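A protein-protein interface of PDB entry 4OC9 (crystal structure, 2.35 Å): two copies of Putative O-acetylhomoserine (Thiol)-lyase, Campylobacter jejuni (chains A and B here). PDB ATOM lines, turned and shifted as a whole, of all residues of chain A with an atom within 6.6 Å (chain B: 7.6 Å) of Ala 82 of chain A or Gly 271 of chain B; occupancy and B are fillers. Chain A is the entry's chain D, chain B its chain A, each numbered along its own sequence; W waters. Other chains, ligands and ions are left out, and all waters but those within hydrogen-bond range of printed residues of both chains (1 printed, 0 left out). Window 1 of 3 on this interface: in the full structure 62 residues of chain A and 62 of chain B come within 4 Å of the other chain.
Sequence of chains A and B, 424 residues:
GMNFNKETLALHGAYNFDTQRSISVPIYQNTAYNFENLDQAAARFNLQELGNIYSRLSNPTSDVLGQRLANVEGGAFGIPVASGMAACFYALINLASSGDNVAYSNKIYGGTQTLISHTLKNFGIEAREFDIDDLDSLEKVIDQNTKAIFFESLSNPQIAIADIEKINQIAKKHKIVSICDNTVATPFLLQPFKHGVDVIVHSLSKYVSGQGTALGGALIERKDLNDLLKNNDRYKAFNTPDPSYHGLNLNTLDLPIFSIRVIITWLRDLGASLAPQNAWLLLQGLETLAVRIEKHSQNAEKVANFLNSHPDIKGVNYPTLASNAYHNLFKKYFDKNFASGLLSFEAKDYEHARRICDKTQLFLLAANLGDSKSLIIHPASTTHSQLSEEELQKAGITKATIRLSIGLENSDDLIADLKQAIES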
ATOM      1  N   PRO A  80     -17.195  25.059  17.645  1.00  0.00           N
ATOM      2  CA  PRO A  80     -18.472  25.652  17.325  1.00  0.00           C
ATOM      3  C   PRO A  80     -19.598  24.694  17.592  1.00  0.00           C
ATOM      4  O   PRO A  80     -19.472  23.499  17.359  1.00  0.00           O
ATOM      5  CB  PRO A  80     -18.356  25.947  15.824  1.00  0.00           C
ATOM      6  CG  PRO A  80     -16.892  25.992  15.568  1.00  0.00           C
ATOM      7  CD  PRO A  80     -16.382  24.877  16.427  1.00  0.00           C
ATOM      8  N   VAL A  81     -20.694  25.269  18.039  1.00  0.00           N
ATOM      9  CA  VAL A  81     -21.887  24.548  18.366  1.00  0.00           C
ATOM     10  C   VAL A  81     -23.107  25.254  17.785  1.00  0.00           C
ATOM     11  O   VAL A  81     -22.989  26.345  17.247  1.00  0.00           O
ATOM     12  CB  VAL A  81     -21.995  24.306  19.875  1.00  0.00           C
ATOM     13  CG1 VAL A  81     -20.879  23.395  20.303  1.00  0.00           C
ATOM     14  CG2 VAL A  81     -21.934  25.590  20.639  1.00  0.00           C
ATOM     15  N   ALA A  82     -24.283  24.629  17.892  1.00  0.00           N
ATOM     16  CA  ALA A  82     -25.518  25.190  17.285  1.00  0.00           C
ATOM     17  C   ALA A  82     -25.958  26.586  17.678  1.00  0.00           C
ATOM     18  O   ALA A  82     -26.672  27.225  16.939  1.00  0.00           O
ATOM     19  CB  ALA A  82     -26.665  24.227  17.476  1.00  0.00           C
ATOM     20  N   SER A  83     -25.604  27.009  18.879  1.00  0.00           N
ATOM     21  CA  SER A  83     -25.991  28.328  19.332  1.00  0.00           C
ATOM     22  C   SER A  83     -25.197  28.747  20.528  1.00  0.00           C
ATOM     23  O   SER A  83     -24.503  27.963  21.124  1.00  0.00           O
ATOM     24  CB  SER A  83     -27.448  28.343  19.745  1.00  0.00           C
ATOM     25  OG  SER A  83     -27.655  27.550  20.895  1.00  0.00           O
ATOM     26  N   GLY A  84     -25.288  30.042  20.826  1.00  0.00           N
ATOM     27  CA  GLY A  84     -24.602  30.656  21.967  1.00  0.00           C
ATOM     28  C   GLY A  84     -25.075  29.997  23.266  1.00  0.00           C
ATOM     29  O   GLY A  84     -24.287  29.732  24.151  1.00  0.00           O
ATOM     30  N   MET A  85     -26.366  29.718  23.356  1.00  0.00           N
ATOM     31  CA  MET A  85     -26.921  29.065  24.538  1.00  0.00           C
ATOM     32  C   MET A  85     -26.311  27.707  24.664  1.00  0.00           C
ATOM     33  O   MET A  85     -25.872  27.321  25.737  1.00  0.00           O
ATOM     34  CB  MET A  85     -28.422  28.873  24.432  1.00  0.00           C
ATOM     35  CG  MET A  85     -29.222  30.152  24.619  1.00  0.00           C
ATOM     36  SD  MET A  85     -28.661  31.162  26.231  1.00  0.00           S
ATOM     37  CE  MET A  85     -28.925  29.737  27.549  1.00  0.00           C
ATOM     38  N   ALA A  86     -26.262  26.964  23.565  1.00  0.00           N
ATOM     39  CA  ALA A  86     -25.673  25.641  23.591  1.00  0.00           C
ATOM     40  C   ALA A  86     -24.240  25.732  24.064  1.00  0.00           C
ATOM     41  O   ALA A  86     -23.779  24.870  24.809  1.00  0.00           O
ATOM     42  CB  ALA A  86     -25.728  24.988  22.225  1.00  0.00           C
ATOM     43  N   ALA A  87     -23.526  26.768  23.640  1.00  0.00           N
ATOM     44  CA  ALA A  87     -22.138  26.976  24.062  1.00  0.00           C
ATOM     45  C   ALA A  87     -22.071  27.208  25.587  1.00  0.00           C
ATOM     46  O   ALA A  87     -21.182  26.673  26.262  1.00  0.00           O
ATOM     47  CB  ALA A  87     -21.524  28.158  23.323  1.00  0.00           C
ATOM     48  N   PHE A  89     -24.331  26.299  27.858  1.00  0.00           N
ATOM     49  CA  PHE A  89     -24.758  25.019  28.439  1.00  0.00           C
ATOM     50  C   PHE A  89     -23.601  24.000  28.448  1.00  0.00           C
ATOM     51  O   PHE A  89     -23.253  23.454  29.494  1.00  0.00           O
ATOM     52  CB  PHE A  89     -26.023  24.552  27.740  1.00  0.00           C
ATOM     53  CG  PHE A  89     -26.390  23.151  28.031  1.00  0.00           C
ATOM     54  CD1 PHE A  89     -26.619  22.735  29.316  1.00  0.00           C
ATOM     55  CD2 PHE A  89     -26.644  22.269  26.979  1.00  0.00           C
ATOM     56  CE1 PHE A  89     -27.001  21.424  29.575  1.00  0.00           C
ATOM     57  CE2 PHE A  89     -27.043  20.979  27.210  1.00  0.00           C
ATOM     58  CZ  PHE A  89     -27.223  20.544  28.524  1.00  0.00           C
ATOM     59  N1  LLP A 206     -24.855  35.428  25.682  1.00  0.00           N
ATOM     60  C2  LLP A 206     -24.949  36.669  25.163  1.00  0.00           C
ATOM     61  C2' LLP A 206     -24.205  37.800  25.770  1.00  0.00           C
ATOM     62  C3  LLP A 206     -25.732  36.899  24.080  1.00  0.00           C
ATOM     63  O3  LLP A 206     -25.741  38.149  23.606  1.00  0.00           O
ATOM     64  C4  LLP A 206     -26.469  35.879  23.469  1.00  0.00           C
ATOM     65  C4' LLP A 206     -27.297  36.128  22.266  1.00  0.00           C
ATOM     66  C5  LLP A 206     -26.368  34.602  23.972  1.00  0.00           C
ATOM     67  C6  LLP A 206     -25.557  34.422  25.106  1.00  0.00           C
ATOM     68  C5' LLP A 206     -27.115  33.401  23.377  1.00  0.00           C
ATOM     69  OP4 LLP A 206     -26.787  33.225  22.005  1.00  0.00           O
ATOM     70  P   LLP A 206     -27.776  32.485  20.965  1.00  0.00           P
ATOM     71  OP1 LLP A 206     -28.255  31.214  21.636  1.00  0.00           O
ATOM     72  OP2 LLP A 206     -26.799  32.237  19.851  1.00  0.00           O
ATOM     73  OP3 LLP A 206     -28.897  33.459  20.675  1.00  0.00           O
ATOM     74  N   LLP A 206     -24.530  36.755  17.112  1.00  0.00           N
ATOM     75  CA  LLP A 206     -24.540  38.200  17.192  1.00  0.00           C
ATOM     76  CB  LLP A 206     -24.443  38.492  18.703  1.00  0.00           C
ATOM     77  CG  LLP A 206     -25.697  38.405  19.605  1.00  0.00           C
ATOM     78  CD  LLP A 206     -27.011  37.610  19.377  1.00  0.00           C
ATOM     79  CE  LLP A 206     -28.044  37.710  20.574  1.00  0.00           C
ATOM     80  NZ  LLP A 206     -27.335  37.315  21.788  1.00  0.00           N
ATOM     81  C   LLP A 206     -23.530  38.919  16.273  1.00  0.00           C
ATOM     82  O   LLP A 206     -23.770  39.028  15.076  1.00  0.00           O
ATOM     83  N   LEU A 215     -27.374  31.553  13.183  1.00  0.00           N
ATOM     84  CA  LEU A 215     -27.392  31.256  14.562  1.00  0.00           C
ATOM     85  C   LEU A 215     -26.169  30.361  14.802  1.00  0.00           C
ATOM     86  O   LEU A 215     -25.886  29.463  14.026  1.00  0.00           O
ATOM     87  CB  LEU A 215     -28.682  30.474  14.899  1.00  0.00           C
ATOM     88  CG  LEU A 215     -28.961  30.258  16.396  1.00  0.00           C
ATOM     89  CD1 LEU A 215     -29.203  31.624  17.032  1.00  0.00           C
ATOM     90  CD2 LEU A 215     -30.170  29.375  16.607  1.00  0.00           C
ATOM     91  N   GLY A 216     -25.478  30.571  15.899  1.00  0.00           N
ATOM     92  CA  GLY A 216     -24.301  29.771  16.245  1.00  0.00           C
ATOM     93  C   GLY A 216     -23.585  30.183  17.524  1.00  0.00           C
ATOM     94  O   GLY A 216     -23.755  31.268  18.026  1.00  0.00           O
ATOM     95  N   GLY A 217     -22.786  29.268  18.054  1.00  0.00           N
ATOM     96  CA  GLY A 217     -22.014  29.512  19.259  1.00  0.00           C
ATOM     97  C   GLY A 217     -20.649  28.849  19.233  1.00  0.00           C
ATOM     98  O   GLY A 217     -20.352  28.038  18.357  1.00  0.00           O
ATOM     99  N   LEU A 267     -21.136  16.843  22.310  1.00  0.00           N
ATOM    100  CA  LEU A 267     -21.604  16.896  20.933  1.00  0.00           C
ATOM    101  C   LEU A 267     -22.083  15.507  20.527  1.00  0.00           C
ATOM    102  O   LEU A 267     -23.168  15.363  19.996  1.00  0.00           O
ATOM    103  CB  LEU A 267     -20.540  17.373  19.930  1.00  0.00           C
ATOM    104  CG  LEU A 267     -20.307  18.864  19.831  1.00  0.00           C
ATOM    105  CD1 LEU A 267     -19.081  19.209  19.002  1.00  0.00           C
ATOM    106  CD2 LEU A 267     -21.562  19.499  19.235  1.00  0.00           C
ATOM    107  N   GLY A 271     -25.743  16.339  20.972  1.00  0.00           N
ATOM    108  CA  GLY A 271     -25.916  16.801  19.604  1.00  0.00           C
ATOM    109  C   GLY A 271     -26.328  18.175  19.165  1.00  0.00           C
ATOM    110  O   GLY A 271     -27.119  18.294  18.223  1.00  0.00           O
ATOM    111  N   ALA A 272     -25.812  19.194  19.827  1.00  0.00           N
ATOM    112  CA  ALA A 272     -26.115  20.580  19.486  1.00  0.00           C
ATOM    113  C   ALA A 272     -25.059  21.019  18.469  1.00  0.00           C
ATOM    114  O   ALA A 272     -24.291  21.946  18.664  1.00  0.00           O
ATOM    115  CB  ALA A 272     -26.088  21.456  20.705  1.00  0.00           C
ATOM    116  N   SER A 273     -25.074  20.324  17.362  1.00  0.00           N
ATOM    117  CA  SER A 273     -24.146  20.524  16.284  1.00  0.00           C
ATOM    118  C   SER A 273     -24.454  21.708  15.370  1.00  0.00           C
ATOM    119  O   SER A 273     -25.602  22.053  15.055  1.00  0.00           O
ATOM    120  CB  SER A 273     -23.969  19.150  15.609  1.00  0.00           C
ATOM    121  OG  SER A 273     -23.053  19.092  14.534  1.00  0.00           O
ATOM    122  N   LEU A 274     -23.390  22.380  14.994  1.00  0.00           N
ATOM    123  CA  LEU A 274     -23.512  23.529  14.128  1.00  0.00           C
ATOM    124  C   LEU A 274     -23.546  23.068  12.666  1.00  0.00           C
ATOM    125  O   LEU A 274     -22.588  22.466  12.177  1.00  0.00           O
ATOM    126  CB  LEU A 274     -22.335  24.498  14.331  1.00  0.00           C
ATOM    127  CG  LEU A 274     -22.395  25.787  13.482  1.00  0.00           C
ATOM    128  CD1 LEU A 274     -23.621  26.626  13.827  1.00  0.00           C
ATOM    129  CD2 LEU A 274     -21.149  26.639  13.667  1.00  0.00           C
ATOM    130  N   ALA A 275     -24.611  23.421  11.965  1.00  0.00           N
ATOM    131  CA  ALA A 275     -24.732  23.086  10.559  1.00  0.00           C
ATOM    132  C   ALA A 275     -23.643  23.775   9.711  1.00  0.00           C
ATOM    133  O   ALA A 275     -23.226  24.902   9.988  1.00  0.00           O
ATOM    134  CB  ALA A 275     -26.101  23.468  10.053  1.00  0.00           C
ATOM    135  N   ASN A 278     -24.240  27.337   8.285  1.00  0.00           N
ATOM    136  CA  ASN A 278     -24.116  28.367   9.326  1.00  0.00           C
ATOM    137  C   ASN A 278     -22.662  28.596   9.656  1.00  0.00           C
ATOM    138  O   ASN A 278     -22.205  29.763   9.752  1.00  0.00           O
ATOM    139  CB  ASN A 278     -24.916  28.089  10.591  1.00  0.00           C
ATOM    140  CG  ASN A 278     -26.402  28.303  10.414  1.00  0.00           C
ATOM    141  OD1 ASN A 278     -26.967  28.111   9.354  1.00  0.00           O
ATOM    142  ND2 ASN A 278     -27.058  28.702  11.504  1.00  0.00           N
ATOM    143  N   ARG B  56     -33.703  30.626  17.448  1.00  0.00           N
ATOM    144  CA  ARG B  56     -33.258  29.559  18.339  1.00  0.00           C
ATOM    145  C   ARG B  56     -34.473  28.772  18.817  1.00  0.00           C
ATOM    146  O   ARG B  56     -34.356  27.588  19.120  1.00  0.00           O
ATOM    147  CB  ARG B  56     -32.402  30.077  19.499  1.00  0.00           C
ATOM    148  CG  ARG B  56     -32.275  29.128  20.681  1.00  0.00           C
ATOM    149  CD  ARG B  56     -31.178  29.465  21.662  1.00  0.00           C
ATOM    150  NE  ARG B  56     -30.897  30.892  21.831  1.00  0.00           N
ATOM    151  CZ  ARG B  56     -31.482  31.745  22.659  1.00  0.00           C
ATOM    152  NH1 ARG B  56     -32.508  31.389  23.419  1.00  0.00           N
ATOM    153  NH2 ARG B  56     -31.027  32.983  22.697  1.00  0.00           N
ATOM    154  N   LEU B  57     -35.629  29.440  18.858  1.00  0.00           N
ATOM    155  CA  LEU B  57     -36.868  28.815  19.305  1.00  0.00           C
ATOM    156  C   LEU B  57     -37.624  28.213  18.127  1.00  0.00           C
ATOM    157  O   LEU B  57     -38.075  27.053  18.204  1.00  0.00           O
ATOM    158  CB  LEU B  57     -37.802  29.824  19.964  1.00  0.00           C
ATOM    159  CG  LEU B  57     -37.188  30.716  21.030  1.00  0.00           C
ATOM    160  CD1 LEU B  57     -38.322  31.370  21.784  1.00  0.00           C
ATOM    161  CD2 LEU B  57     -36.386  29.894  21.976  1.00  0.00           C
ATOM    162  N   VAL B  81     -35.034  19.699  15.493  1.00  0.00           N
ATOM    163  CA  VAL B  81     -33.907  20.084  16.289  1.00  0.00           C
ATOM    164  C   VAL B  81     -32.611  19.799  15.526  1.00  0.00           C
ATOM    165  O   VAL B  81     -32.644  19.175  14.477  1.00  0.00           O
ATOM    166  CB  VAL B  81     -33.956  19.421  17.666  1.00  0.00           C
ATOM    167  CG1 VAL B  81     -35.145  19.942  18.406  1.00  0.00           C
ATOM    168  CG2 VAL B  81     -34.048  17.925  17.557  1.00  0.00           C
ATOM    169  N   ALA B  82     -31.473  20.195  16.099  1.00  0.00           N
ATOM    170  CA  ALA B  82     -30.168  20.032  15.435  1.00  0.00           C
ATOM    171  C   ALA B  82     -29.733  18.645  15.016  1.00  0.00           C
ATOM    172  O   ALA B  82     -28.923  18.514  14.106  1.00  0.00           O
ATOM    173  CB  ALA B  82     -29.064  20.667  16.257  1.00  0.00           C
ATOM    174  N   ALA B  86     -30.040  14.986  19.628  1.00  0.00           N
ATOM    175  CA  ALA B  86     -30.675  16.079  20.348  1.00  0.00           C
ATOM    176  C   ALA B  86     -32.147  15.777  20.534  1.00  0.00           C
ATOM    177  O   ALA B  86     -32.704  16.088  21.579  1.00  0.00           O
ATOM    178  CB  ALA B  86     -30.496  17.396  19.627  1.00  0.00           C
ATOM    179  N   TYR B  90     -33.767  15.630  24.156  1.00  0.00           N
ATOM    180  CA  TYR B  90     -34.907  16.507  24.432  1.00  0.00           C
ATOM    181  C   TYR B  90     -36.160  15.764  24.805  1.00  0.00           C
ATOM    182  O   TYR B  90     -36.897  16.204  25.682  1.00  0.00           O
ATOM    183  CB  TYR B  90     -35.144  17.427  23.226  1.00  0.00           C
ATOM    184  CG  TYR B  90     -34.283  18.673  23.215  1.00  0.00           C
ATOM    185  CD1 TYR B  90     -32.971  18.663  23.725  1.00  0.00           C
ATOM    186  CD2 TYR B  90     -34.692  19.826  22.519  1.00  0.00           C
ATOM    187  CE1 TYR B  90     -32.170  19.809  23.703  1.00  0.00           C
ATOM    188  CE2 TYR B  90     -33.878  20.968  22.467  1.00  0.00           C
ATOM    189  CZ  TYR B  90     -32.618  20.945  23.042  1.00  0.00           C
ATOM    190  OH  TYR B  90     -31.814  22.036  23.014  1.00  0.00           O
ATOM    191  N   VAL B 262     -40.815  21.771  24.968  1.00  0.00           N
ATOM    192  CA  VAL B 262     -39.578  21.588  24.186  1.00  0.00           C
ATOM    193  C   VAL B 262     -39.091  22.937  23.633  1.00  0.00           C
ATOM    194  O   VAL B 262     -37.911  23.247  23.624  1.00  0.00           O
ATOM    195  CB  VAL B 262     -39.785  20.650  22.979  1.00  0.00           C
ATOM    196  CG1 VAL B 262     -38.531  20.614  22.126  1.00  0.00           C
ATOM    197  CG2 VAL B 262     -40.188  19.250  23.428  1.00  0.00           C
ATOM    198  N   THR B 265     -38.597  25.871  26.785  1.00  0.00           N
ATOM    199  CA  THR B 265     -37.578  25.510  27.758  1.00  0.00           C
ATOM    200  C   THR B 265     -36.307  24.875  27.161  1.00  0.00           C
ATOM    201  O   THR B 265     -35.244  25.470  27.232  1.00  0.00           O
ATOM    202  CB  THR B 265     -38.142  24.552  28.851  1.00  0.00           C
ATOM    203  OG1 THR B 265     -39.290  25.155  29.458  1.00  0.00           O
ATOM    204  CG2 THR B 265     -37.101  24.237  29.887  1.00  0.00           C
ATOM    205  N   TRP B 266     -36.422  23.726  26.509  1.00  0.00           N
ATOM    206  CA  TRP B 266     -35.231  23.051  25.966  1.00  0.00           C
ATOM    207  C   TRP B 266     -34.544  23.747  24.777  1.00  0.00           C
ATOM    208  O   TRP B 266     -33.333  23.808  24.728  1.00  0.00           O
ATOM    209  CB  TRP B 266     -35.548  21.596  25.710  1.00  0.00           C
ATOM    210  CG  TRP B 266     -36.207  20.949  26.932  1.00  0.00           C
ATOM    211  CD1 TRP B 266     -37.477  20.434  27.002  1.00  0.00           C
ATOM    212  CD2 TRP B 266     -35.699  20.900  28.271  1.00  0.00           C
ATOM    213  NE1 TRP B 266     -37.753  20.007  28.267  1.00  0.00           N
ATOM    214  CE2 TRP B 266     -36.683  20.284  29.070  1.00  0.00           C
ATOM    215  CE3 TRP B 266     -34.504  21.309  28.867  1.00  0.00           C
ATOM    216  CZ2 TRP B 266     -36.508  20.054  30.422  1.00  0.00           C
ATOM    217  CZ3 TRP B 266     -34.322  21.073  30.218  1.00  0.00           C
ATOM    218  CH2 TRP B 266     -35.317  20.449  30.982  1.00  0.00           C
ATOM    219  N   LEU B 267     -35.316  24.196  23.788  1.00  0.00           N
ATOM    220  CA  LEU B 267     -34.706  24.916  22.672  1.00  0.00           C
ATOM    221  C   LEU B 267     -34.245  26.261  23.170  1.00  0.00           C
ATOM    222  O   LEU B 267     -33.115  26.654  22.954  1.00  0.00           O
ATOM    223  CB  LEU B 267     -35.642  25.124  21.484  1.00  0.00           C
ATOM    224  CG  LEU B 267     -35.812  23.957  20.528  1.00  0.00           C
ATOM    225  CD1 LEU B 267     -36.931  24.187  19.531  1.00  0.00           C
ATOM    226  CD2 LEU B 267     -34.486  23.737  19.806  1.00  0.00           C
ATOM    227  N   ARG B 268     -35.105  26.929  23.919  1.00  0.00           N
ATOM    228  CA  ARG B 268     -34.754  28.252  24.410  1.00  0.00           C
ATOM    229  C   ARG B 268     -33.527  28.308  25.292  1.00  0.00           C
ATOM    230  O   ARG B 268     -32.697  29.198  25.113  1.00  0.00           O
ATOM    231  CB  ARG B 268     -35.931  28.895  25.152  1.00  0.00           C
ATOM    232  CG  ARG B 268     -35.659  30.333  25.530  1.00  0.00           C
ATOM    233  CD  ARG B 268     -36.894  31.010  26.069  1.00  0.00           C
ATOM    234  NE  ARG B 268     -36.688  32.459  26.185  1.00  0.00           N
ATOM    235  CZ  ARG B 268     -37.602  33.336  26.607  1.00  0.00           C
ATOM    236  NH1 ARG B 268     -38.822  32.948  26.962  1.00  0.00           N
ATOM    237  NH2 ARG B 268     -37.292  34.627  26.677  1.00  0.00           N
ATOM    238  N   ASP B 269     -33.407  27.374  26.226  1.00  0.00           N
ATOM    239  CA  ASP B 269     -32.274  27.386  27.140  1.00  0.00           C
ATOM    240  C   ASP B 269     -31.088  26.477  26.793  1.00  0.00           C
ATOM    241  O   ASP B 269     -29.955  26.802  27.130  1.00  0.00           O
ATOM    242  CB  ASP B 269     -32.765  27.061  28.546  1.00  0.00           C
ATOM    243  CG  ASP B 269     -33.879  28.014  29.038  1.00  0.00           C
ATOM    244  OD1 ASP B 269     -34.150  29.045  28.396  1.00  0.00           O
ATOM    245  OD2 ASP B 269     -34.507  27.705  30.076  1.00  0.00           O
ATOM    246  N   LEU B 270     -31.320  25.344  26.145  1.00  0.00           N
ATOM    247  CA  LEU B 270     -30.218  24.431  25.794  1.00  0.00           C
ATOM    248  C   LEU B 270     -29.722  24.708  24.346  1.00  0.00           C
ATOM    249  O   LEU B 270     -28.580  24.400  23.978  1.00  0.00           O
ATOM    250  CB  LEU B 270     -30.568  22.956  26.028  1.00  0.00           C
ATOM    251  CG  LEU B 270     -30.984  22.360  27.378  1.00  0.00           C
ATOM    252  CD1 LEU B 270     -30.877  20.843  27.763  1.00  0.00           C
ATOM    253  CD2 LEU B 270     -30.041  23.106  28.253  1.00  0.00           C
ATOM    254  N   GLY B 271     -30.610  25.235  23.513  1.00  0.00           N
ATOM    255  CA  GLY B 271     -30.261  25.607  22.143  1.00  0.00           C
ATOM    256  C   GLY B 271     -29.755  24.681  21.052  1.00  0.00           C
ATOM    257  O   GLY B 271     -28.894  25.099  20.278  1.00  0.00           O
ATOM    258  N   ALA B 272     -30.310  23.489  20.953  1.00  0.00           N
ATOM    259  CA  ALA B 272     -29.930  22.536  19.917  1.00  0.00           C
ATOM    260  C   ALA B 272     -30.853  22.796  18.707  1.00  0.00           C
ATOM    261  O   ALA B 272     -31.632  21.954  18.262  1.00  0.00           O
ATOM    262  CB  ALA B 272     -30.080  21.123  20.405  1.00  0.00           C
ATOM    263  N   SER B 273     -30.756  24.016  18.209  1.00  0.00           N
ATOM    264  CA  SER B 273     -31.566  24.493  17.100  1.00  0.00           C
ATOM    265  C   SER B 273     -31.138  24.000  15.698  1.00  0.00           C
ATOM    266  O   SER B 273     -29.948  23.858  15.380  1.00  0.00           O
ATOM    267  CB  SER B 273     -31.712  26.010  17.297  1.00  0.00           C
ATOM    268  OG  SER B 273     -32.524  26.692  16.348  1.00  0.00           O
ATOM    269  N   LEU B 274     -32.142  23.693  14.883  1.00  0.00           N
ATOM    270  CA  LEU B 274     -31.917  23.211  13.535  1.00  0.00           C
ATOM    271  C   LEU B 274     -31.758  24.410  12.601  1.00  0.00           C
ATOM    272  O   LEU B 274     -32.663  25.249  12.471  1.00  0.00           O
ATOM    273  CB  LEU B 274     -33.077  22.342  13.058  1.00  0.00           C
ATOM    274  CG  LEU B 274     -32.866  21.784  11.650  1.00  0.00           C
ATOM    275  CD1 LEU B 274     -31.658  20.864  11.588  1.00  0.00           C
ATOM    276  CD2 LEU B 274     -34.080  21.019  11.179  1.00  0.00           C
ATOM    277  N   ALA B 275     -30.614  24.487  11.945  1.00  0.00           N
ATOM    278  CA  ALA B 275     -30.358  25.578  11.018  1.00  0.00           C
ATOM    279  C   ALA B 275     -31.336  25.532   9.835  1.00  0.00           C
ATOM    280  O   ALA B 275     -31.720  24.463   9.370  1.00  0.00           O
ATOM    281  CB  ALA B 275     -28.922  25.517  10.535  1.00  0.00           C
HETATM  282  O   HOH W   1     -26.958  20.107  12.525  1.00  0.00           O
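The backbone carbonyl oxygen (O) of Gly 271 of chain B sits at hydrogen-bond distance from the side-chain hydroxyl (OG) of Ser 83 of chain A (2.8 Å). OP1 of LLP 206 of chain A sits close to the guanidinium group of Arg 56 of chain B (2.7 Å). N of Ala 86 of chain A lies close to O of Leu 270 of chain B (3.5 Å).
The backbone carbonyl oxygen (O) of Ala 272 of chain A sits at hydrogen-bond distance from the backbone NH (N) of Ala 82 of chain A (2.8 Å). The side-chain hydroxyl (OG) of Ser 83 of chain A is in hydrogen-bond range of the backbone NH (N) of Ala 86 of chain A, 3.1 Å away. O of Trp 266 of chain B lies within hydrogen-bond range of N of Gly 271 of chain B, at 3.3 Å. O of Leu 215 of chain A lies within hydrogen-bond range of ND2 of Asn 278 of chain A, at 2.9 Å. The side-chain hydroxyl (OH) of Tyr 90 of chain B sits at hydrogen-bond distance from the backbone NH (N) of Gly 271 of chain B (3.5 Å). The backbone NH (N) of Ala 82 of chain B lies within hydrogen-bond range of the backbone carbonyl oxygen (O) of Ala 272 of chain B (2.8 Å).
Ala 82 of chain A touches Gly 271 of chain B (CB to O, 3.7 Å). Ala 82 of chain A touches Ser 273 of chain B. CG of Met 85 of chain A touches O of Arg 268 of chain B, 3.6 Å away. CE of Met 85 of chain A touches O of Asp 269 of chain B, at 3.1 Å. Ala 86 of chain A touches Gly 271 of chain B (CB to O, 3.7 Å). Phe 89 of chain A touches Leu 270 of chain B (CD1 to CD2, 3.6 Å). Leu 215 of chain A touches Ser 273 of chain B. Ser 273 of chain A touches Ala 82 of chain B (O to CB, 3.9 Å). CB of Ala 275 of chain B touches CB of Ala 275 of chain A, 3.5 Å away. Ala 275 of chain B touches Asn 278 of chain A.
Printed residues of chain B within 4 Å of Ala 82 of chain A: Gly 271 and Ser 273. Printed residues of chain B within 4 Å of LLP 206 of chain A: Arg 56. Printed residues of chain A within 4 Å of Asp 269 of chain B: Met 85 (3.1 Å). Of the printed residues of chain B, Leu 215 of chain A touches Arg 56 (3.5 Å) and Ser 273 (3.6 Å). Of the printed residues of chain A, Leu 270 of chain B touches Ala 86 (3.2 Å) and Phe 89 (3.6 Å). Printed residues of chain B within 4 Å of Met 85 of chain A: Arg 56, Arg 268 and Asp 269. Thr 265 of chain B touches none of the printed residues of chain A. The nearest printed residue of chain B that does not touch Ala 82 of chain A is Ala 272 of chain B (4.4 Å). The nearest printed residue of chain A that does not touch Ser 273 of chain B is Ser 273 of chain A (4.7 Å).
Hydrophobic or aromatic side chains of chain A within 4 Å of the printed part of chain B: Ala 82, Met 85, Ala 86, Phe 89, Leu 215 and Ala 275. Of the 18 printed residues of chain B, 9 touch a printed residue of chain A. Hydrophobic or aromatic side chains of chain B that line the printed part of chain A: Ala 82, Ala 86, Leu 270 and Ala 275. Among the printed residues, 17 pairs touch across the chains. Among the printed residues, no Asp or Glu carboxylate lies within 4 Å of a Lys or Arg side-chain nitrogen of the other chain.
Ala 82 of chain A touches Gly 271 of chain B, and with the chains exchanged Gly 271 of chain A touches Ala 82 of chain B. Ala 82 of chain A touches Ser 273 of chain B, and with the chains exchanged Ser 273 of chain A touches Ala 82 of chain B. Ala 86 of chain A touches Gly 271 of chain B, and with the chains exchanged Gly 271 of chain A touches Ala 86 of chain B. Ala 275 of chain B touches its own counterpart, Ala 275 of chain A. 9 positions are printed for both chains.
Water W1 bridges O of Ala 82 of chain B (3.0 Å) and O of Ser 273 of chain A (3.5 Å).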
